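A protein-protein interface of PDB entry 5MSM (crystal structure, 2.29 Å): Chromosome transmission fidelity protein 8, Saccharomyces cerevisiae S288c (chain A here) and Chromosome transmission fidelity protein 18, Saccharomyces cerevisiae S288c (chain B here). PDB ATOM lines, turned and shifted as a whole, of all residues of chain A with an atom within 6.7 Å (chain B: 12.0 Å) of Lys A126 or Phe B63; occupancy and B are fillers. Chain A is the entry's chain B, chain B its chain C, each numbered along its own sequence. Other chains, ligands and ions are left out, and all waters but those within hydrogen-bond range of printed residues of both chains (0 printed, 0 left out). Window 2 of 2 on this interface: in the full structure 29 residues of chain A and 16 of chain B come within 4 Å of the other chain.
The side-chain hydroxyl of Tyr B59 is in hydrogen-bond range of the side-chain amide nitrogen of Gln A36. The side-chain amide nitrogen of Gln A36 sits at hydrogen-bond distance from the backbone carbonyl oxygen of Asn B60 (2.8 Å). The backbone NH (N) of Arg A128 sits close to the side-chain hydroxyl (OH) of Tyr B59 (3.5 Å). The side-chain carboxylate (OE2) of Glu B61 is in salt-bridge range of the guanidinium group (NH2) of Arg A128 (2.9 Å). The backbone carbonyl oxygen of Lys A126 lies close to the side-chain hydroxyl of Tyr B59 (2.3 Å).
N of Gln A36 is in hydrogen-bond range of O of Phe A125 (2.9 Å). NZ of Lys A126 sits close to OE1 of Gln A36, 3.2 Å away.
Among the printed residues, pairs that only touch across the chains: Gln A36 with Glu B61 (3.5 Å), Gln A36 with Gly B62 (3.5 Å), Lys A126 with Phe B63 (3.9 Å) and Asp A127 with Tyr B59 (3.4 Å).
Ile A35 touches none of the printed residues of chain B. Of the printed residues of chain B, Gln A36 touches Tyr B59 (3.1 Å), Asn B60 (2.8 Å), Glu B61 (3.5 Å) and Gly B62 (3.5 Å). No residue of chain B comes within 4 Å of Gly A92. No residue of chain B comes within 4 Å of Ile A124. No residue of chain B comes within 4 Å of Phe A125. Lys A126 touches just these residues of chain B: Tyr B59 and Phe B63. Asp A127 touches just one residue of chain B: Tyr B59. Printed residues of chain B within 4 Å of Arg A128: Tyr B59 and Glu B61. Printed residues of chain A within 4 Å of Asn B60: Gln A36 (2.8 Å). Of the printed residues of chain A, Gly B62 touches Gln A36 (3.5 Å). Of the printed residues of chain A, Phe B63 touches Lys A126 (3.9 Å). Ala B66 touches none of the printed residues of chain A. The nearest residue of chain B that does not touch Lys A126 is Asn B60 (5.2 Å). The nearest residue of chain A that does not touch Phe B63 is Gln A36 (4.3 Å).
Hydrophobic or aromatic side chains of chain B within 4 Å of the printed part of chain A: Tyr B59 and Phe B63.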
ATOM      1  N   GLU A  34     -33.592  -9.984 -25.895  1.00  0.00           N
ATOM      2  CA  GLU A  34     -32.647  -9.818 -24.795  1.00  0.00           C
ATOM      3  C   GLU A  34     -31.202  -9.892 -25.275  1.00  0.00           C
ATOM      4  O   GLU A  34     -30.815 -10.779 -26.056  1.00  0.00           O
ATOM      5  CB  GLU A  34     -32.924 -10.864 -23.684  1.00  0.00           C
ATOM      6  CG  GLU A  34     -31.953 -10.794 -22.498  1.00  0.00           C
ATOM      7  CD  GLU A  34     -32.459 -11.505 -21.253  1.00  0.00           C
ATOM      8  OE1 GLU A  34     -33.597 -12.038 -21.291  1.00  0.00           O
ATOM      9  OE2 GLU A  34     -31.732 -11.490 -20.222  1.00  0.00           O
ATOM     10  N   ILE A  35     -30.396  -8.951 -24.793  1.00  0.00           N
ATOM     11  CA  ILE A  35     -29.002  -8.833 -25.204  1.00  0.00           C
ATOM     12  C   ILE A  35     -28.092  -8.622 -24.008  1.00  0.00           C
ATOM     13  O   ILE A  35     -28.375  -7.776 -23.165  1.00  0.00           O
ATOM     14  CB  ILE A  35     -28.819  -7.647 -26.178  1.00  0.00           C
ATOM     15  CG1 ILE A  35     -29.708  -7.802 -27.421  1.00  0.00           C
ATOM     16  CG2 ILE A  35     -27.380  -7.470 -26.552  1.00  0.00           C
ATOM     17  CD1 ILE A  35     -29.995  -6.480 -28.120  1.00  0.00           C
ATOM     18  N   GLN A  36     -26.989  -9.364 -23.941  1.00  0.00           N
ATOM     19  CA  GLN A  36     -26.003  -9.151 -22.882  1.00  0.00           C
ATOM     20  C   GLN A  36     -25.094  -7.963 -23.195  1.00  0.00           C
ATOM     21  O   GLN A  36     -23.957  -8.137 -23.612  1.00  0.00           O
ATOM     22  CB  GLN A  36     -25.161 -10.394 -22.679  1.00  0.00           C
ATOM     23  CG  GLN A  36     -24.444 -10.424 -21.351  1.00  0.00           C
ATOM     24  CD  GLN A  36     -23.670 -11.698 -21.176  1.00  0.00           C
ATOM     25  OE1 GLN A  36     -24.236 -12.747 -20.860  1.00  0.00           O
ATOM     26  NE2 GLN A  36     -22.362 -11.630 -21.411  1.00  0.00           N
ATOM     27  N   LEU A  90     -24.471 -10.915 -34.052  1.00  0.00           N
ATOM     28  CA  LEU A  90     -24.528 -11.590 -32.750  1.00  0.00           C
ATOM     29  C   LEU A  90     -25.272 -12.893 -32.859  1.00  0.00           C
ATOM     30  O   LEU A  90     -26.377 -12.911 -33.392  1.00  0.00           O
ATOM     31  CB  LEU A  90     -25.211 -10.713 -31.709  1.00  0.00           C
ATOM     32  CG  LEU A  90     -24.475  -9.463 -31.232  1.00  0.00           C
ATOM     33  CD1 LEU A  90     -24.532  -8.327 -32.237  1.00  0.00           C
ATOM     34  CD2 LEU A  90     -25.082  -9.023 -29.899  1.00  0.00           C
ATOM     35  N   LEU A  91     -24.704 -13.975 -32.332  1.00  0.00           N
ATOM     36  CA  LEU A  91     -25.387 -15.264 -32.439  1.00  0.00           C
ATOM     37  C   LEU A  91     -26.145 -15.598 -31.159  1.00  0.00           C
ATOM     38  O   LEU A  91     -25.611 -15.477 -30.058  1.00  0.00           O
ATOM     39  CB  LEU A  91     -24.401 -16.397 -32.773  1.00  0.00           C
ATOM     40  CG  LEU A  91     -23.590 -16.238 -34.071  1.00  0.00           C
ATOM     41  CD1 LEU A  91     -22.701 -17.463 -34.331  1.00  0.00           C
ATOM     42  CD2 LEU A  91     -24.510 -15.950 -35.257  1.00  0.00           C
ATOM     43  N   GLY A  92     -27.399 -16.003 -31.311  1.00  0.00           N
ATOM     44  CA  GLY A  92     -28.225 -16.269 -30.161  1.00  0.00           C
ATOM     45  C   GLY A  92     -29.185 -17.420 -30.314  1.00  0.00           C
ATOM     46  O   GLY A  92     -29.031 -18.280 -31.176  1.00  0.00           O
ATOM     47  N   LYS A  93     -30.197 -17.400 -29.460  1.00  0.00           N
ATOM     48  CA  LYS A  93     -31.044 -18.545 -29.197  1.00  0.00           C
ATOM     49  C   LYS A  93     -32.497 -18.118 -28.908  1.00  0.00           C
ATOM     50  O   LYS A  93     -32.747 -17.097 -28.255  1.00  0.00           O
ATOM     51  CB  LYS A  93     -30.415 -19.307 -28.023  1.00  0.00           C
ATOM     52  CG  LYS A  93     -31.255 -20.322 -27.337  1.00  0.00           C
ATOM     53  CD  LYS A  93     -30.492 -20.867 -26.134  1.00  0.00           C
ATOM     54  CE  LYS A  93     -31.190 -22.096 -25.539  1.00  0.00           C
ATOM     55  NZ  LYS A  93     -32.466 -21.772 -24.813  1.00  0.00           N
ATOM     56  N   ILE A 124     -32.580 -14.361 -27.157  1.00  0.00           N
ATOM     57  CA  ILE A 124     -31.531 -13.837 -26.291  1.00  0.00           C
ATOM     58  C   ILE A 124     -30.159 -14.004 -26.910  1.00  0.00           C
ATOM     59  O   ILE A 124     -29.892 -15.022 -27.558  1.00  0.00           O
ATOM     60  CB  ILE A 124     -31.557 -14.541 -24.911  1.00  0.00           C
ATOM     61  CG1 ILE A 124     -30.487 -13.997 -23.975  1.00  0.00           C
ATOM     62  CG2 ILE A 124     -31.407 -16.050 -25.055  1.00  0.00           C
ATOM     63  CD1 ILE A 124     -30.822 -14.251 -22.501  1.00  0.00           C
ATOM     64  N   PHE A 125     -29.299 -13.005 -26.701  1.00  0.00           N
ATOM     65  CA  PHE A 125     -27.945 -12.986 -27.270  1.00  0.00           C
ATOM     66  C   PHE A 125     -26.917 -12.718 -26.175  1.00  0.00           C
ATOM     67  O   PHE A 125     -26.792 -11.592 -25.711  1.00  0.00           O
ATOM     68  CB  PHE A 125     -27.853 -11.926 -28.410  1.00  0.00           C
ATOM     69  CG  PHE A 125     -28.780 -12.221 -29.554  1.00  0.00           C
ATOM     70  CD1 PHE A 125     -30.087 -11.765 -29.536  1.00  0.00           C
ATOM     71  CD2 PHE A 125     -28.354 -13.002 -30.630  1.00  0.00           C
ATOM     72  CE1 PHE A 125     -30.961 -12.075 -30.564  1.00  0.00           C
ATOM     73  CE2 PHE A 125     -29.217 -13.319 -31.679  1.00  0.00           C
ATOM     74  CZ  PHE A 125     -30.517 -12.859 -31.656  1.00  0.00           C
ATOM     75  N   LYS A 126     -26.167 -13.754 -25.798  1.00  0.00           N
ATOM     76  CA  LYS A 126     -25.261 -13.745 -24.644  1.00  0.00           C
ATOM     77  C   LYS A 126     -23.787 -13.563 -25.068  1.00  0.00           C
ATOM     78  O   LYS A 126     -22.913 -13.262 -24.243  1.00  0.00           O
ATOM     79  CB  LYS A 126     -25.388 -15.053 -23.847  1.00  0.00           C
ATOM     80  CG  LYS A 126     -26.806 -15.426 -23.409  1.00  0.00           C
ATOM     81  CD  LYS A 126     -27.040 -15.284 -21.880  1.00  0.00           C
ATOM     82  CE  LYS A 126     -27.079 -13.798 -21.396  1.00  0.00           C
ATOM     83  NZ  LYS A 126     -27.204 -13.559 -19.900  1.00  0.00           N
ATOM     84  N   ASP A 127     -23.503 -13.765 -26.353  1.00  0.00           N
ATOM     85  CA  ASP A 127     -22.113 -13.850 -26.787  1.00  0.00           C
ATOM     86  C   ASP A 127     -21.591 -12.605 -27.480  1.00  0.00           C
ATOM     87  O   ASP A 127     -22.358 -11.886 -28.111  1.00  0.00           O
ATOM     88  CB  ASP A 127     -21.988 -15.065 -27.684  1.00  0.00           C
ATOM     89  CG  ASP A 127     -21.971 -16.334 -26.882  1.00  0.00           C
ATOM     90  OD1 ASP A 127     -20.903 -16.638 -26.313  1.00  0.00           O
ATOM     91  OD2 ASP A 127     -23.041 -16.958 -26.721  1.00  0.00           O
ATOM     92  N   ARG A 128     -20.286 -12.362 -27.332  1.00  0.00           N
ATOM     93  CA  ARG A 128     -19.594 -11.234 -27.956  1.00  0.00           C
ATOM     94  C   ARG A 128     -20.030 -11.079 -29.416  1.00  0.00           C
ATOM     95  O   ARG A 128     -20.206 -12.076 -30.125  1.00  0.00           O
ATOM     96  CB  ARG A 128     -18.076 -11.431 -27.886  1.00  0.00           C
ATOM     97  CG  ARG A 128     -17.262 -10.156 -27.958  1.00  0.00           C
ATOM     98  CD  ARG A 128     -15.772 -10.473 -27.825  1.00  0.00           C
ATOM     99  NE  ARG A 128     -15.540 -11.238 -26.604  1.00  0.00           N
ATOM    100  CZ  ARG A 128     -15.380 -10.706 -25.391  1.00  0.00           C
ATOM    101  NH1 ARG A 128     -15.380  -9.383 -25.232  1.00  0.00           N
ATOM    102  NH2 ARG A 128     -15.191 -11.503 -24.340  1.00  0.00           N
ATOM    103  N   VAL B  57     -23.913  -2.754 -30.395  1.00  0.00           N
ATOM    104  CA  VAL B  57     -23.962  -3.308 -29.045  1.00  0.00           C
ATOM    105  C   VAL B  57     -22.611  -3.193 -28.348  1.00  0.00           C
ATOM    106  O   VAL B  57     -21.624  -3.778 -28.812  1.00  0.00           O
ATOM    107  CB  VAL B  57     -24.363  -4.796 -29.066  1.00  0.00           C
ATOM    108  CG1 VAL B  57     -24.123  -5.450 -27.715  1.00  0.00           C
ATOM    109  CG2 VAL B  57     -25.807  -4.947 -29.484  1.00  0.00           C
ATOM    110  N   LYS B  58     -22.559  -2.470 -27.230  1.00  0.00           N
ATOM    111  CA  LYS B  58     -21.402  -2.567 -26.343  1.00  0.00           C
ATOM    112  C   LYS B  58     -21.618  -3.764 -25.436  1.00  0.00           C
ATOM    113  O   LYS B  58     -22.447  -3.724 -24.531  1.00  0.00           O
ATOM    114  CB  LYS B  58     -21.191  -1.323 -25.482  1.00  0.00           C
ATOM    115  CG  LYS B  58     -20.106  -1.562 -24.438  1.00  0.00           C
ATOM    116  CD  LYS B  58     -20.459  -1.013 -23.075  1.00  0.00           C
ATOM    117  CE  LYS B  58     -19.768  -1.825 -21.965  1.00  0.00           C
ATOM    118  NZ  LYS B  58     -18.270  -1.786 -22.072  1.00  0.00           N
ATOM    119  N   TYR B  59     -20.879  -4.827 -25.700  1.00  0.00           N
ATOM    120  CA  TYR B  59     -21.017  -6.088 -24.995  1.00  0.00           C
ATOM    121  C   TYR B  59     -20.716  -6.005 -23.498  1.00  0.00           C
ATOM    122  O   TYR B  59     -19.790  -5.324 -23.084  1.00  0.00           O
ATOM    123  CB  TYR B  59     -20.119  -7.130 -25.667  1.00  0.00           C
ATOM    124  CG  TYR B  59     -20.294  -8.546 -25.171  1.00  0.00           C
ATOM    125  CD1 TYR B  59     -21.504  -9.193 -25.292  1.00  0.00           C
ATOM    126  CD2 TYR B  59     -19.228  -9.252 -24.619  1.00  0.00           C
ATOM    127  CE1 TYR B  59     -21.666 -10.491 -24.860  1.00  0.00           C
ATOM    128  CE2 TYR B  59     -19.389 -10.555 -24.177  1.00  0.00           C
ATOM    129  CZ  TYR B  59     -20.612 -11.166 -24.311  1.00  0.00           C
ATOM    130  OH  TYR B  59     -20.796 -12.470 -23.903  1.00  0.00           O
ATOM    131  N   ASN B  60     -21.514  -6.699 -22.690  1.00  0.00           N
ATOM    132  CA  ASN B  60     -21.164  -6.883 -21.282  1.00  0.00           C
ATOM    133  C   ASN B  60     -20.480  -8.216 -21.163  1.00  0.00           C
ATOM    134  O   ASN B  60     -20.937  -9.189 -21.765  1.00  0.00           O
ATOM    135  CB  ASN B  60     -22.393  -6.840 -20.379  1.00  0.00           C
ATOM    136  CG  ASN B  60     -23.052  -5.492 -20.356  1.00  0.00           C
ATOM    137  OD1 ASN B  60     -22.405  -4.461 -20.540  1.00  0.00           O
ATOM    138  ND2 ASN B  60     -24.368  -5.488 -20.157  1.00  0.00           N
ATOM    139  N   GLU B  61     -19.395  -8.267 -20.393  1.00  0.00           N
ATOM    140  CA  GLU B  61     -18.596  -9.475 -20.320  1.00  0.00           C
ATOM    141  C   GLU B  61     -19.367 -10.595 -19.644  1.00  0.00           C
ATOM    142  O   GLU B  61     -19.163 -11.768 -19.926  1.00  0.00           O
ATOM    143  CB  GLU B  61     -17.279  -9.207 -19.590  1.00  0.00           C
ATOM    144  CG  GLU B  61     -16.374  -8.251 -20.324  1.00  0.00           C
ATOM    145  CD  GLU B  61     -16.010  -8.756 -21.728  1.00  0.00           C
ATOM    146  OE1 GLU B  61     -15.848  -7.908 -22.642  1.00  0.00           O
ATOM    147  OE2 GLU B  61     -15.891  -9.992 -21.916  1.00  0.00           O
ATOM    148  N   GLY B  62     -20.237 -10.230 -18.716  1.00  0.00           N
ATOM    149  CA  GLY B  62     -21.148 -11.196 -18.148  1.00  0.00           C
ATOM    150  C   GLY B  62     -22.446 -10.564 -17.693  1.00  0.00           C
ATOM    151  O   GLY B  62     -22.908  -9.596 -18.284  1.00  0.00           O
ATOM    152  N   PHE B  63     -23.040 -11.135 -16.651  1.00  0.00           N
ATOM    153  CA  PHE B  63     -24.418 -10.831 -16.276  1.00  0.00           C
ATOM    154  C   PHE B  63     -24.558 -10.705 -14.749  1.00  0.00           C
ATOM    155  O   PHE B  63     -24.111 -11.582 -14.000  1.00  0.00           O
ATOM    156  CB  PHE B  63     -25.385 -11.908 -16.832  1.00  0.00           C
ATOM    157  CG  PHE B  63     -26.821 -11.754 -16.360  1.00  0.00           C
ATOM    158  CD1 PHE B  63     -27.645 -10.757 -16.892  1.00  0.00           C
ATOM    159  CD2 PHE B  63     -27.354 -12.608 -15.389  1.00  0.00           C
ATOM    160  CE1 PHE B  63     -28.983 -10.613 -16.468  1.00  0.00           C
ATOM    161  CE2 PHE B  63     -28.672 -12.459 -14.952  1.00  0.00           C
ATOM    162  CZ  PHE B  63     -29.485 -11.450 -15.493  1.00  0.00           C
ATOM    163  N   SER B  64     -25.186  -9.612 -14.314  1.00  0.00           N
ATOM    164  CA  SER B  64     -25.483  -9.347 -12.908  1.00  0.00           C
ATOM    165  C   SER B  64     -26.978  -9.227 -12.719  1.00  0.00           C
ATOM    166  O   SER B  64     -27.649  -8.449 -13.411  1.00  0.00           O
ATOM    167  CB  SER B  64     -24.844  -8.049 -12.430  1.00  0.00           C
ATOM    168  OG  SER B  64     -23.449  -8.162 -12.228  1.00  0.00           O
ATOM    169  N   ASN B  65     -27.465 -10.009 -11.765  1.00  0.00           N
ATOM    170  CA  ASN B  65     -28.826 -10.042 -11.268  1.00  0.00           C
ATOM    171  C   ASN B  65     -28.694  -9.456  -9.873  1.00  0.00           C
ATOM    172  O   ASN B  65     -27.922  -9.976  -9.077  1.00  0.00           O
ATOM    173  CB  ASN B  65     -29.336 -11.488 -11.210  1.00  0.00           C
ATOM    174  CG  ASN B  65     -30.694 -11.700 -11.862  1.00  0.00           C
ATOM    175  OD1 ASN B  65     -31.485 -10.775 -12.045  1.00  0.00           O
ATOM    176  ND2 ASN B  65     -30.997 -12.957 -12.150  1.00  0.00           N
ATOM    177  N   ALA B  66     -29.381  -8.366  -9.565  1.00  0.00           N
ATOM    178  CA  ALA B  66     -29.178  -7.752  -8.260  1.00  0.00           C
ATOM    179  C   ALA B  66     -30.030  -8.449  -7.199  1.00  0.00           C
ATOM    180  O   ALA B  66     -30.786  -9.375  -7.495  1.00  0.00           O
ATOM    181  CB  ALA B  66     -29.484  -6.244  -8.303  1.00  0.00           C
ATOM    182  N   VAL B  67     -29.878  -8.019  -5.951  1.00  0.00           N
ATOM    183  CA  VAL B  67     -30.639  -8.593  -4.862  1.00  0.00           C
ATOM    184  C   VAL B  67     -32.099  -8.174  -5.062  1.00  0.00           C
ATOM    185  O   VAL B  67     -32.357  -7.064  -5.534  1.00  0.00           O
ATOM    186  CB  VAL B  67     -30.071  -8.100  -3.492  1.00  0.00           C
ATOM    187  CG1 VAL B  67     -31.174  -7.606  -2.578  1.00  0.00           C
ATOM    188  CG2 VAL B  67     -29.194  -9.175  -2.830  1.00  0.00           C
ATOM    189  N   ARG B  68     -33.057  -9.032  -4.730  1.00  0.00           N
ATOM    190  CA  ARG B  68     -34.448  -8.611  -4.853  1.00  0.00           C
ATOM    191  C   ARG B  68     -34.839  -7.570  -3.787  1.00  0.00           C
ATOM    192  O   ARG B  68     -34.301  -7.551  -2.677  1.00  0.00           O
ATOM    193  CB  ARG B  68     -35.402  -9.811  -4.793  1.00  0.00           C
ATOM    194  CG  ARG B  68     -35.554 -10.489  -3.440  1.00  0.00           C
ATOM    195  CD  ARG B  68     -36.693 -11.544  -3.476  1.00  0.00           C
ATOM    196  NE  ARG B  68     -36.954 -12.310  -2.236  1.00  0.00           N
ATOM    197  CZ  ARG B  68     -36.940 -11.848  -0.979  1.00  0.00           C
ATOM    198  NH1 ARG B  68     -36.656 -10.571  -0.684  1.00  0.00           N
ATOM    199  NH2 ARG B  68     -37.218 -12.694   0.012  1.00  0.00           N
